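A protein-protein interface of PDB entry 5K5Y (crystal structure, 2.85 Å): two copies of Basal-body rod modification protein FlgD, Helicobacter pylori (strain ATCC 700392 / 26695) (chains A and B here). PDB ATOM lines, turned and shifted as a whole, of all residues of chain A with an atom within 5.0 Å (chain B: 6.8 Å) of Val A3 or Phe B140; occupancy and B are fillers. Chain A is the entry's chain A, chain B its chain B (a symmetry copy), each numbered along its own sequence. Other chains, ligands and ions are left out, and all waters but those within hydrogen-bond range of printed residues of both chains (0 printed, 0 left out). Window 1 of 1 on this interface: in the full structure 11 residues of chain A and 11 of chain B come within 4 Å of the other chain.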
ATOM      1  N   ASN A   1      32.090  26.818 -15.234  1.00  0.00           N
ATOM      2  CA  ASN A   1      31.633  26.135 -13.974  1.00  0.00           C
ATOM      3  C   ASN A   1      30.538  26.839 -13.140  1.00  0.00           C
ATOM      4  O   ASN A   1      29.931  26.157 -12.320  1.00  0.00           O
ATOM      5  CB  ASN A   1      32.831  25.807 -13.041  1.00  0.00           C
ATOM      6  CG  ASN A   1      33.771  24.743 -13.611  1.00  0.00           C
ATOM      7  OD1 ASN A   1      33.349  23.818 -14.305  1.00  0.00           O
ATOM      8  ND2 ASN A   1      35.056  24.865 -13.299  1.00  0.00           N
ATOM      9  N   SER A   2      30.335  28.159 -13.283  1.00  0.00           N
ATOM     10  CA  SER A   2      29.337  28.904 -12.488  1.00  0.00           C
ATOM     11  C   SER A   2      28.035  29.257 -13.193  1.00  0.00           C
ATOM     12  O   SER A   2      28.039  29.927 -14.214  1.00  0.00           O
ATOM     13  CB  SER A   2      29.974  30.200 -11.982  1.00  0.00           C
ATOM     14  OG  SER A   2      29.244  30.725 -10.927  1.00  0.00           O
ATOM     15  N   VAL A   3      26.937  28.837 -12.565  1.00  0.00           N
ATOM     16  CA  VAL A   3      25.576  29.132 -12.998  1.00  0.00           C
ATOM     17  C   VAL A   3      24.829  29.929 -11.929  1.00  0.00           C
ATOM     18  O   VAL A   3      23.608  30.043 -11.953  1.00  0.00           O
ATOM     19  CB  VAL A   3      24.791  27.837 -13.282  1.00  0.00           C
ATOM     20  CG1 VAL A   3      25.552  26.952 -14.256  1.00  0.00           C
ATOM     21  CG2 VAL A   3      24.473  27.046 -12.017  1.00  0.00           C
ATOM     22  N   SER A   4      25.579  30.524 -11.011  1.00  0.00           N
ATOM     23  CA  SER A   4      25.024  31.357  -9.936  1.00  0.00           C
ATOM     24  C   SER A   4      24.217  32.546 -10.419  1.00  0.00           C
ATOM     25  O   SER A   4      23.295  33.012  -9.754  1.00  0.00           O
ATOM     26  CB  SER A   4      26.140  31.907  -9.046  1.00  0.00           C
ATOM     27  OG  SER A   4      27.025  32.734  -9.753  1.00  0.00           O
ATOM     28  N   MET A   5      24.585  33.060 -11.572  1.00  0.00           N
ATOM     29  CA  MET A   5      23.813  34.117 -12.265  1.00  0.00           C
ATOM     30  C   MET A   5      22.326  33.804 -12.530  1.00  0.00           C
ATOM     31  O   MET A   5      21.462  34.610 -12.284  1.00  0.00           O
ATOM     32  CB  MET A   5      24.557  34.504 -13.516  1.00  0.00           C
ATOM     33  CG  MET A   5      24.975  33.397 -14.462  1.00  0.00           C
ATOM     34  SD  MET A   5      26.612  33.811 -15.181  1.00  0.00           S
ATOM     35  CE  MET A   5      27.720  33.168 -13.929  1.00  0.00           C
ATOM     36  N   ILE A   6      22.017  32.562 -12.855  1.00  0.00           N
ATOM     37  CA  ILE A   6      20.621  32.216 -13.143  1.00  0.00           C
ATOM     38  C   ILE A   6      19.737  32.870 -12.103  1.00  0.00           C
ATOM     39  O   ILE A   6      19.968  32.711 -10.911  1.00  0.00           O
ATOM     40  CB  ILE A   6      20.311  30.714 -13.074  1.00  0.00           C
ATOM     41  CG1 ILE A   6      21.120  29.927 -14.117  1.00  0.00           C
ATOM     42  CG2 ILE A   6      18.822  30.472 -13.350  1.00  0.00           C
ATOM     43  CD1 ILE A   6      21.061  28.417 -13.982  1.00  0.00           C
ATOM     44  N   GLU A 114      17.549  33.441 -17.563  1.00  0.00           N
ATOM     45  CA  GLU A 114      16.535  32.391 -17.361  1.00  0.00           C
ATOM     46  C   GLU A 114      17.121  30.967 -17.315  1.00  0.00           C
ATOM     47  O   GLU A 114      16.583  30.061 -16.638  1.00  0.00           O
ATOM     48  CB  GLU A 114      15.452  32.502 -18.434  1.00  0.00           C
ATOM     49  CG  GLU A 114      14.641  33.787 -18.338  1.00  0.00           C
ATOM     50  CD  GLU A 114      13.613  33.896 -19.428  1.00  0.00           C
ATOM     51  OE1 GLU A 114      13.958  33.634 -20.615  1.00  0.00           O
ATOM     52  OE2 GLU A 114      12.471  34.265 -19.111  1.00  0.00           O
ATOM     53  N   SER A 115      18.215  30.781 -18.044  1.00  0.00           N
ATOM     54  CA  SER A 115      18.930  29.512 -18.024  1.00  0.00           C
ATOM     55  C   SER A 115      20.396  29.728 -18.418  1.00  0.00           C
ATOM     56  O   SER A 115      20.765  30.799 -18.887  1.00  0.00           O
ATOM     57  CB  SER A 115      18.231  28.503 -18.942  1.00  0.00           C
ATOM     58  OG  SER A 115      18.553  28.721 -20.293  1.00  0.00           O
ATOM     59  N   VAL A 116      21.227  28.723 -18.186  1.00  0.00           N
ATOM     60  CA  VAL A 116      22.611  28.732 -18.653  1.00  0.00           C
ATOM     61  C   VAL A 116      22.822  27.490 -19.508  1.00  0.00           C
ATOM     62  O   VAL A 116      22.502  26.381 -19.085  1.00  0.00           O
ATOM     63  CB  VAL A 116      23.629  28.747 -17.505  1.00  0.00           C
ATOM     64  CG1 VAL A 116      25.049  28.532 -18.016  1.00  0.00           C
ATOM     65  CG2 VAL A 116      23.556  30.058 -16.767  1.00  0.00           C
ATOM     66  N   PHE A 118      25.414  25.183 -22.246  1.00  0.00           N
ATOM     67  CA  PHE A 118      26.788  24.872 -22.642  1.00  0.00           C
ATOM     68  C   PHE A 118      26.762  24.414 -24.083  1.00  0.00           C
ATOM     69  O   PHE A 118      26.236  23.335 -24.374  1.00  0.00           O
ATOM     70  CB  PHE A 118      27.384  23.844 -21.717  1.00  0.00           C
ATOM     71  CG  PHE A 118      27.659  24.386 -20.354  1.00  0.00           C
ATOM     72  CD1 PHE A 118      26.651  24.486 -19.408  1.00  0.00           C
ATOM     73  CD2 PHE A 118      28.916  24.858 -20.018  1.00  0.00           C
ATOM     74  CE1 PHE A 118      26.908  25.027 -18.136  1.00  0.00           C
ATOM     75  CE2 PHE A 118      29.180  25.391 -18.746  1.00  0.00           C
ATOM     76  CZ  PHE A 118      28.179  25.477 -17.802  1.00  0.00           C
ATOM     77  N   SER B   2      32.659  25.661  -8.054  1.00  0.00           N
ATOM     78  CA  SER B   2      31.238  26.101  -7.989  1.00  0.00           C
ATOM     79  C   SER B   2      30.165  24.977  -7.845  1.00  0.00           C
ATOM     80  O   SER B   2      30.104  23.990  -8.600  1.00  0.00           O
ATOM     81  CB  SER B   2      30.909  27.058  -9.129  1.00  0.00           C
ATOM     82  OG  SER B   2      30.829  26.367 -10.315  1.00  0.00           O
ATOM     83  N   VAL B   3      29.343  25.175  -6.818  1.00  0.00           N
ATOM     84  CA  VAL B   3      28.236  24.297  -6.449  1.00  0.00           C
ATOM     85  C   VAL B   3      26.914  25.053  -6.585  1.00  0.00           C
ATOM     86  O   VAL B   3      25.890  24.654  -6.023  1.00  0.00           O
ATOM     87  CB  VAL B   3      28.399  23.764  -4.989  1.00  0.00           C
ATOM     88  CG1 VAL B   3      29.746  23.087  -4.816  1.00  0.00           C
ATOM     89  CG2 VAL B   3      28.239  24.846  -3.937  1.00  0.00           C
ATOM     90  N   SER B   4      26.957  26.178  -7.300  1.00  0.00           N
ATOM     91  CA  SER B   4      25.780  27.047  -7.518  1.00  0.00           C
ATOM     92  C   SER B   4      24.604  26.305  -8.162  1.00  0.00           C
ATOM     93  O   SER B   4      23.444  26.653  -7.975  1.00  0.00           O
ATOM     94  CB  SER B   4      26.196  28.241  -8.372  1.00  0.00           C
ATOM     95  OG  SER B   4      27.074  27.829  -9.416  1.00  0.00           O
ATOM     96  N   MET B   5      24.946  25.286  -8.928  1.00  0.00           N
ATOM     97  CA  MET B   5      23.985  24.398  -9.562  1.00  0.00           C
ATOM     98  C   MET B   5      23.126  23.549  -8.661  1.00  0.00           C
ATOM     99  O   MET B   5      22.122  23.021  -9.124  1.00  0.00           O
ATOM    100  CB  MET B   5      24.692  23.483 -10.557  1.00  0.00           C
ATOM    101  CG  MET B   5      25.862  22.703  -9.998  1.00  0.00           C
ATOM    102  SD  MET B   5      27.080  22.552 -11.320  1.00  0.00           S
ATOM    103  CE  MET B   5      27.967  24.075 -11.109  1.00  0.00           C
ATOM    104  N   ILE B   6      23.503  23.383  -7.403  1.00  0.00           N
ATOM    105  CA  ILE B   6      22.653  22.645  -6.450  1.00  0.00           C
ATOM    106  C   ILE B   6      21.318  23.347  -6.351  1.00  0.00           C
ATOM    107  O   ILE B   6      21.284  24.522  -6.118  1.00  0.00           O
ATOM    108  CB  ILE B   6      23.229  22.557  -5.017  1.00  0.00           C
ATOM    109  CG1 ILE B   6      24.581  21.816  -4.989  1.00  0.00           C
ATOM    110  CG2 ILE B   6      22.254  21.821  -4.092  1.00  0.00           C
ATOM    111  CD1 ILE B   6      25.341  21.929  -3.681  1.00  0.00           C
ATOM    112  N   LYS B   8      19.160  23.680  -8.836  1.00  0.00           N
ATOM    113  CA  LYS B   8      18.782  23.938 -10.224  1.00  0.00           C
ATOM    114  C   LYS B   8      18.381  22.634 -10.876  1.00  0.00           C
ATOM    115  O   LYS B   8      18.777  21.575 -10.434  1.00  0.00           O
ATOM    116  CB  LYS B   8      19.966  24.494 -11.035  1.00  0.00           C
ATOM    117  CG  LYS B   8      20.656  25.729 -10.492  1.00  0.00           C
ATOM    118  CD  LYS B   8      19.731  26.914 -10.482  1.00  0.00           C
ATOM    119  CE  LYS B   8      20.501  28.146 -10.040  1.00  0.00           C
ATOM    120  NZ  LYS B   8      20.702  28.175  -8.568  1.00  0.00           N
ATOM    121  N   ILE B   9      17.594  22.733 -11.937  1.00  0.00           N
ATOM    122  CA  ILE B   9      17.357  21.622 -12.859  1.00  0.00           C
ATOM    123  C   ILE B   9      18.499  21.565 -13.838  1.00  0.00           C
ATOM    124  O   ILE B   9      18.862  22.576 -14.417  1.00  0.00           O
ATOM    125  CB  ILE B   9      16.036  21.772 -13.659  1.00  0.00           C
ATOM    126  CG1 ILE B   9      14.842  21.915 -12.709  1.00  0.00           C
ATOM    127  CG2 ILE B   9      15.788  20.601 -14.626  1.00  0.00           C
ATOM    128  CD1 ILE B   9      14.758  20.858 -11.643  1.00  0.00           C
ATOM    129  N   ALA B  10      19.017  20.367 -14.042  1.00  0.00           N
ATOM    130  CA  ALA B  10      20.091  20.113 -14.986  1.00  0.00           C
ATOM    131  C   ALA B  10      19.635  19.210 -16.117  1.00  0.00           C
ATOM    132  O   ALA B  10      18.852  18.270 -15.893  1.00  0.00           O
ATOM    133  CB  ALA B  10      21.269  19.476 -14.267  1.00  0.00           C
ATOM    134  N   GLU B  11      20.149  19.481 -17.316  1.00  0.00           N
ATOM    135  CA  GLU B  11      20.018  18.604 -18.493  1.00  0.00           C
ATOM    136  C   GLU B  11      21.404  18.132 -18.889  1.00  0.00           C
ATOM    137  O   GLU B  11      22.333  18.938 -18.994  1.00  0.00           O
ATOM    138  CB  GLU B  11      19.447  19.355 -19.674  1.00  0.00           C
ATOM    139  CG  GLU B  11      18.064  19.949 -19.442  1.00  0.00           C
ATOM    140  CD  GLU B  11      16.909  19.015 -19.795  1.00  0.00           C
ATOM    141  OE1 GLU B  11      17.089  18.053 -20.585  1.00  0.00           O
ATOM    142  OE2 GLU B  11      15.788  19.278 -19.293  1.00  0.00           O
ATOM    143  N   VAL B 113      19.448  18.899  -9.328  1.00  0.00           N
ATOM    144  CA  VAL B 113      20.749  18.573  -8.785  1.00  0.00           C
ATOM    145  C   VAL B 113      20.644  18.604  -7.270  1.00  0.00           C
ATOM    146  O   VAL B 113      20.414  19.653  -6.684  1.00  0.00           O
ATOM    147  CB  VAL B 113      21.775  19.571  -9.268  1.00  0.00           C
ATOM    148  CG1 VAL B 113      23.149  19.294  -8.658  1.00  0.00           C
ATOM    149  CG2 VAL B 113      21.843  19.502 -10.789  1.00  0.00           C
ATOM    150  N   LEU B 125      27.788  15.428 -10.153  1.00  0.00           N
ATOM    151  CA  LEU B 125      26.438  15.839  -9.802  1.00  0.00           C
ATOM    152  C   LEU B 125      25.575  14.673  -9.367  1.00  0.00           C
ATOM    153  O   LEU B 125      25.473  13.694 -10.087  1.00  0.00           O
ATOM    154  CB  LEU B 125      25.763  16.480 -11.027  1.00  0.00           C
ATOM    155  CG  LEU B 125      25.995  17.955 -11.304  1.00  0.00           C
ATOM    156  CD1 LEU B 125      27.453  18.388 -11.174  1.00  0.00           C
ATOM    157  CD2 LEU B 125      25.484  18.244 -12.692  1.00  0.00           C
ATOM    158  N   ILE B 134      30.556  16.722 -14.074  1.00  0.00           N
ATOM    159  CA  ILE B 134      29.975  18.071 -14.324  1.00  0.00           C
ATOM    160  C   ILE B 134      29.974  18.323 -15.813  1.00  0.00           C
ATOM    161  O   ILE B 134      29.060  18.918 -16.335  1.00  0.00           O
ATOM    162  CB  ILE B 134      30.664  19.269 -13.580  1.00  0.00           C
ATOM    163  CG1 ILE B 134      32.061  19.619 -14.153  1.00  0.00           C
ATOM    164  CG2 ILE B 134      30.824  18.945 -12.107  1.00  0.00           C
ATOM    165  CD1 ILE B 134      32.713  20.880 -13.573  1.00  0.00           C
ATOM    166  N   ALA B 137      26.934  17.874 -18.136  1.00  0.00           N
ATOM    167  CA  ALA B 137      25.797  18.783 -18.054  1.00  0.00           C
ATOM    168  C   ALA B 137      25.827  19.795 -19.173  1.00  0.00           C
ATOM    169  O   ALA B 137      26.852  20.460 -19.397  1.00  0.00           O
ATOM    170  CB  ALA B 137      25.812  19.520 -16.735  1.00  0.00           C
ATOM    171  N   ILE B 138      24.697  19.920 -19.858  1.00  0.00           N
ATOM    172  CA  ILE B 138      24.599  20.795 -21.033  1.00  0.00           C
ATOM    173  C   ILE B 138      23.676  21.992 -20.860  1.00  0.00           C
ATOM    174  O   ILE B 138      23.721  22.906 -21.662  1.00  0.00           O
ATOM    175  CB  ILE B 138      24.224  20.015 -22.309  1.00  0.00           C
ATOM    176  CG1 ILE B 138      22.837  19.368 -22.191  1.00  0.00           C
ATOM    177  CG2 ILE B 138      25.284  18.952 -22.573  1.00  0.00           C
ATOM    178  CD1 ILE B 138      22.251  18.903 -23.508  1.00  0.00           C
ATOM    179  N   GLU B 139      22.856  22.005 -19.821  1.00  0.00           N
ATOM    180  CA  GLU B 139      22.023  23.168 -19.535  1.00  0.00           C
ATOM    181  C   GLU B 139      21.528  23.164 -18.099  1.00  0.00           C
ATOM    182  O   GLU B 139      21.338  22.104 -17.496  1.00  0.00           O
ATOM    183  CB  GLU B 139      20.836  23.181 -20.490  1.00  0.00           C
ATOM    184  CG  GLU B 139      19.884  24.350 -20.286  1.00  0.00           C
ATOM    185  CD  GLU B 139      18.697  24.341 -21.235  1.00  0.00           C
ATOM    186  OE1 GLU B 139      18.277  23.243 -21.675  1.00  0.00           O
ATOM    187  OE2 GLU B 139      18.175  25.445 -21.511  1.00  0.00           O
ATOM    188  N   PHE B 140      21.323  24.353 -17.553  1.00  0.00           N
ATOM    189  CA  PHE B 140      20.781  24.534 -16.189  1.00  0.00           C
ATOM    190  C   PHE B 140      19.675  25.573 -16.196  1.00  0.00           C
ATOM    191  O   PHE B 140      19.773  26.576 -16.909  1.00  0.00           O
ATOM    192  CB  PHE B 140      21.880  24.998 -15.204  1.00  0.00           C
ATOM    193  CG  PHE B 140      22.978  23.985 -14.968  1.00  0.00           C
ATOM    194  CD1 PHE B 140      24.099  23.964 -15.770  1.00  0.00           C
ATOM    195  CD2 PHE B 140      22.885  23.046 -13.940  1.00  0.00           C
ATOM    196  CE1 PHE B 140      25.097  23.026 -15.562  1.00  0.00           C
ATOM    197  CE2 PHE B 140      23.885  22.111 -13.717  1.00  0.00           C
ATOM    198  CZ  PHE B 140      24.992  22.101 -14.529  1.00  0.00           C
ATOM    199  N   TYR B 141      18.644  25.367 -15.389  1.00  0.00           N
ATOM    200  CA  TYR B 141      17.609  26.393 -15.185  1.00  0.00           C
ATOM    201  C   TYR B 141      16.882  26.151 -13.862  1.00  0.00           C
ATOM    202  O   TYR B 141      17.074  25.101 -13.265  1.00  0.00           O
ATOM    203  CB  TYR B 141      16.626  26.406 -16.354  1.00  0.00           C
ATOM    204  CG  TYR B 141      16.110  25.051 -16.764  1.00  0.00           C
ATOM    205  CD1 TYR B 141      15.017  24.495 -16.144  1.00  0.00           C
ATOM    206  CD2 TYR B 141      16.711  24.328 -17.787  1.00  0.00           C
ATOM    207  CE1 TYR B 141      14.534  23.238 -16.512  1.00  0.00           C
ATOM    208  CE2 TYR B 141      16.231  23.068 -18.168  1.00  0.00           C
ATOM    209  CZ  TYR B 141      15.138  22.536 -17.526  1.00  0.00           C
ATOM    210  OH  TYR B 141      14.665  21.289 -17.855  1.00  0.00           O
ATOM    211  N   GLN B 142      16.072  27.099 -13.381  1.00  0.00           N
ATOM    212  CA  GLN B 142      15.361  26.878 -12.112  1.00  0.00           C
ATOM    213  C   GLN B 142      14.090  26.078 -12.324  1.00  0.00           C
ATOM    214  O   GLN B 142      13.522  26.109 -13.408  1.00  0.00           O
ATOM    215  CB  GLN B 142      15.002  28.179 -11.413  1.00  0.00           C
ATOM    216  CG  GLN B 142      16.133  28.691 -10.545  1.00  0.00           C
ATOM    217  CD  GLN B 142      16.205  30.201 -10.482  1.00  0.00           C
ATOM    218  OE1 GLN B 142      15.345  30.914 -11.014  1.00  0.00           O
ATOM    219  NE2 GLN B 142      17.256  30.707  -9.836  1.00  0.00           N
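The backbone NH of Ile B138 lies within hydrogen-bond range of the backbone carbonyl oxygen of Glu B11 (2.7 Å).
O of Ser B4 is in hydrogen-bond range of NZ of Lys B8 (3.2 Å).
O of Lys B8 is in hydrogen-bond range of N of Val B113, at 3.0 Å.
The backbone carbonyl oxygen (O) of Glu B139 lies within hydrogen-bond range of the backbone NH (N) of Glu B11, 2.9 Å away.
The side-chain hydroxyl (OH) of Tyr B141 sits at hydrogen-bond distance from the side-chain carboxylate (OE2) of Glu B11, at 2.7 Å.
OG of Ser A4 lies within hydrogen-bond range of OG of Ser A2 (3.2 Å).
Ser B2 touches its own counterpart, Ser A2.
Ser A2 touches Ser B4, but with the chains exchanged Ser A4 does not touch Ser B2 (6.6 Å).
Val A3 touches Met B5, but with the chains exchanged Met A5 does not touch Val B3 (9.7 Å).
Ser B4 touches its own counterpart, Ser A4.
Of the 18 printed residues of chain B, 10 touch a printed residue of chain A.
Printed residues of chain B that touch a printed residue of chain A: Ser B2, Ser B4, Met B5, Lys B8, Ile B134, Ile B138, Glu B139, Phe B140, Tyr B141 and Gln B142.
Of the 10 printed residues of chain A, 9 touch a printed residue of chain B.
Printed residues of chain A that touch a printed residue of chain B: Asn A1, Ser A2, Val A3, Ser A4, Ile A6, Glu A114, Ser A115, Val A116 and Phe A118.
Hydrophobic or aromatic side chains of chain A that line the printed part of chain B: Val A3, Ile A6 and Phe A118.
Among the printed residues, 20 pairs touch across the chains.
O of Asn A1 touches CE of Met B5, 3.1 Å away.
Ser B4 touches Ser A2.
Val A3 touches Phe B140 (CG1 to CD1, 3.7 Å).
Lys B8 touches Ile A6 (CE to CB, 3.98 Å).
Ile A6 touches Phe B140.
Gln B142 touches Ile A6 (NE2 to O, 3.5 Å).
Glu A114 touches Tyr B141.
Ser A115 touches Phe B140.
Glu B139 touches Val A116.
Phe A118 touches Phe B140.
The backbone carbonyl oxygen of Asn A1 lies close to the side-chain hydroxyl of Ser B2.
The backbone NH of Phe B140 sits at hydrogen-bond distance from the backbone carbonyl oxygen of Val A116, at 2.8 Å.
The backbone NH (N) of Val A3 is in hydrogen-bond range of the side-chain hydroxyl (OG) of Ser B4 (3.3 Å).
The backbone NH of Ser A4 sits at hydrogen-bond distance from the side-chain hydroxyl of Ser B4.
N of Phe A118 lies within hydrogen-bond range of O of Ile B138, 2.9 Å away.
Of the printed residues of chain B, Val A3 touches Ser B4, Met B5 and Phe B140.
Printed residues of chain B within 4 Å of Ser A4: Ser B4 (3.5 Å).
Printed residues of chain A within 4 Å of Ser B2: Asn A1 and Ser A2.
Val B113 touches none of the printed residues of chain A.
Printed residues of chain A within 4 Å of Gln B142: Ile A6.
The nearest residue of chain B that does not touch Val A3 is Lys B8 (4.1 Å).
The nearest printed residue of chain A that does not touch Ile B134 is Phe A118 (6.7 Å).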
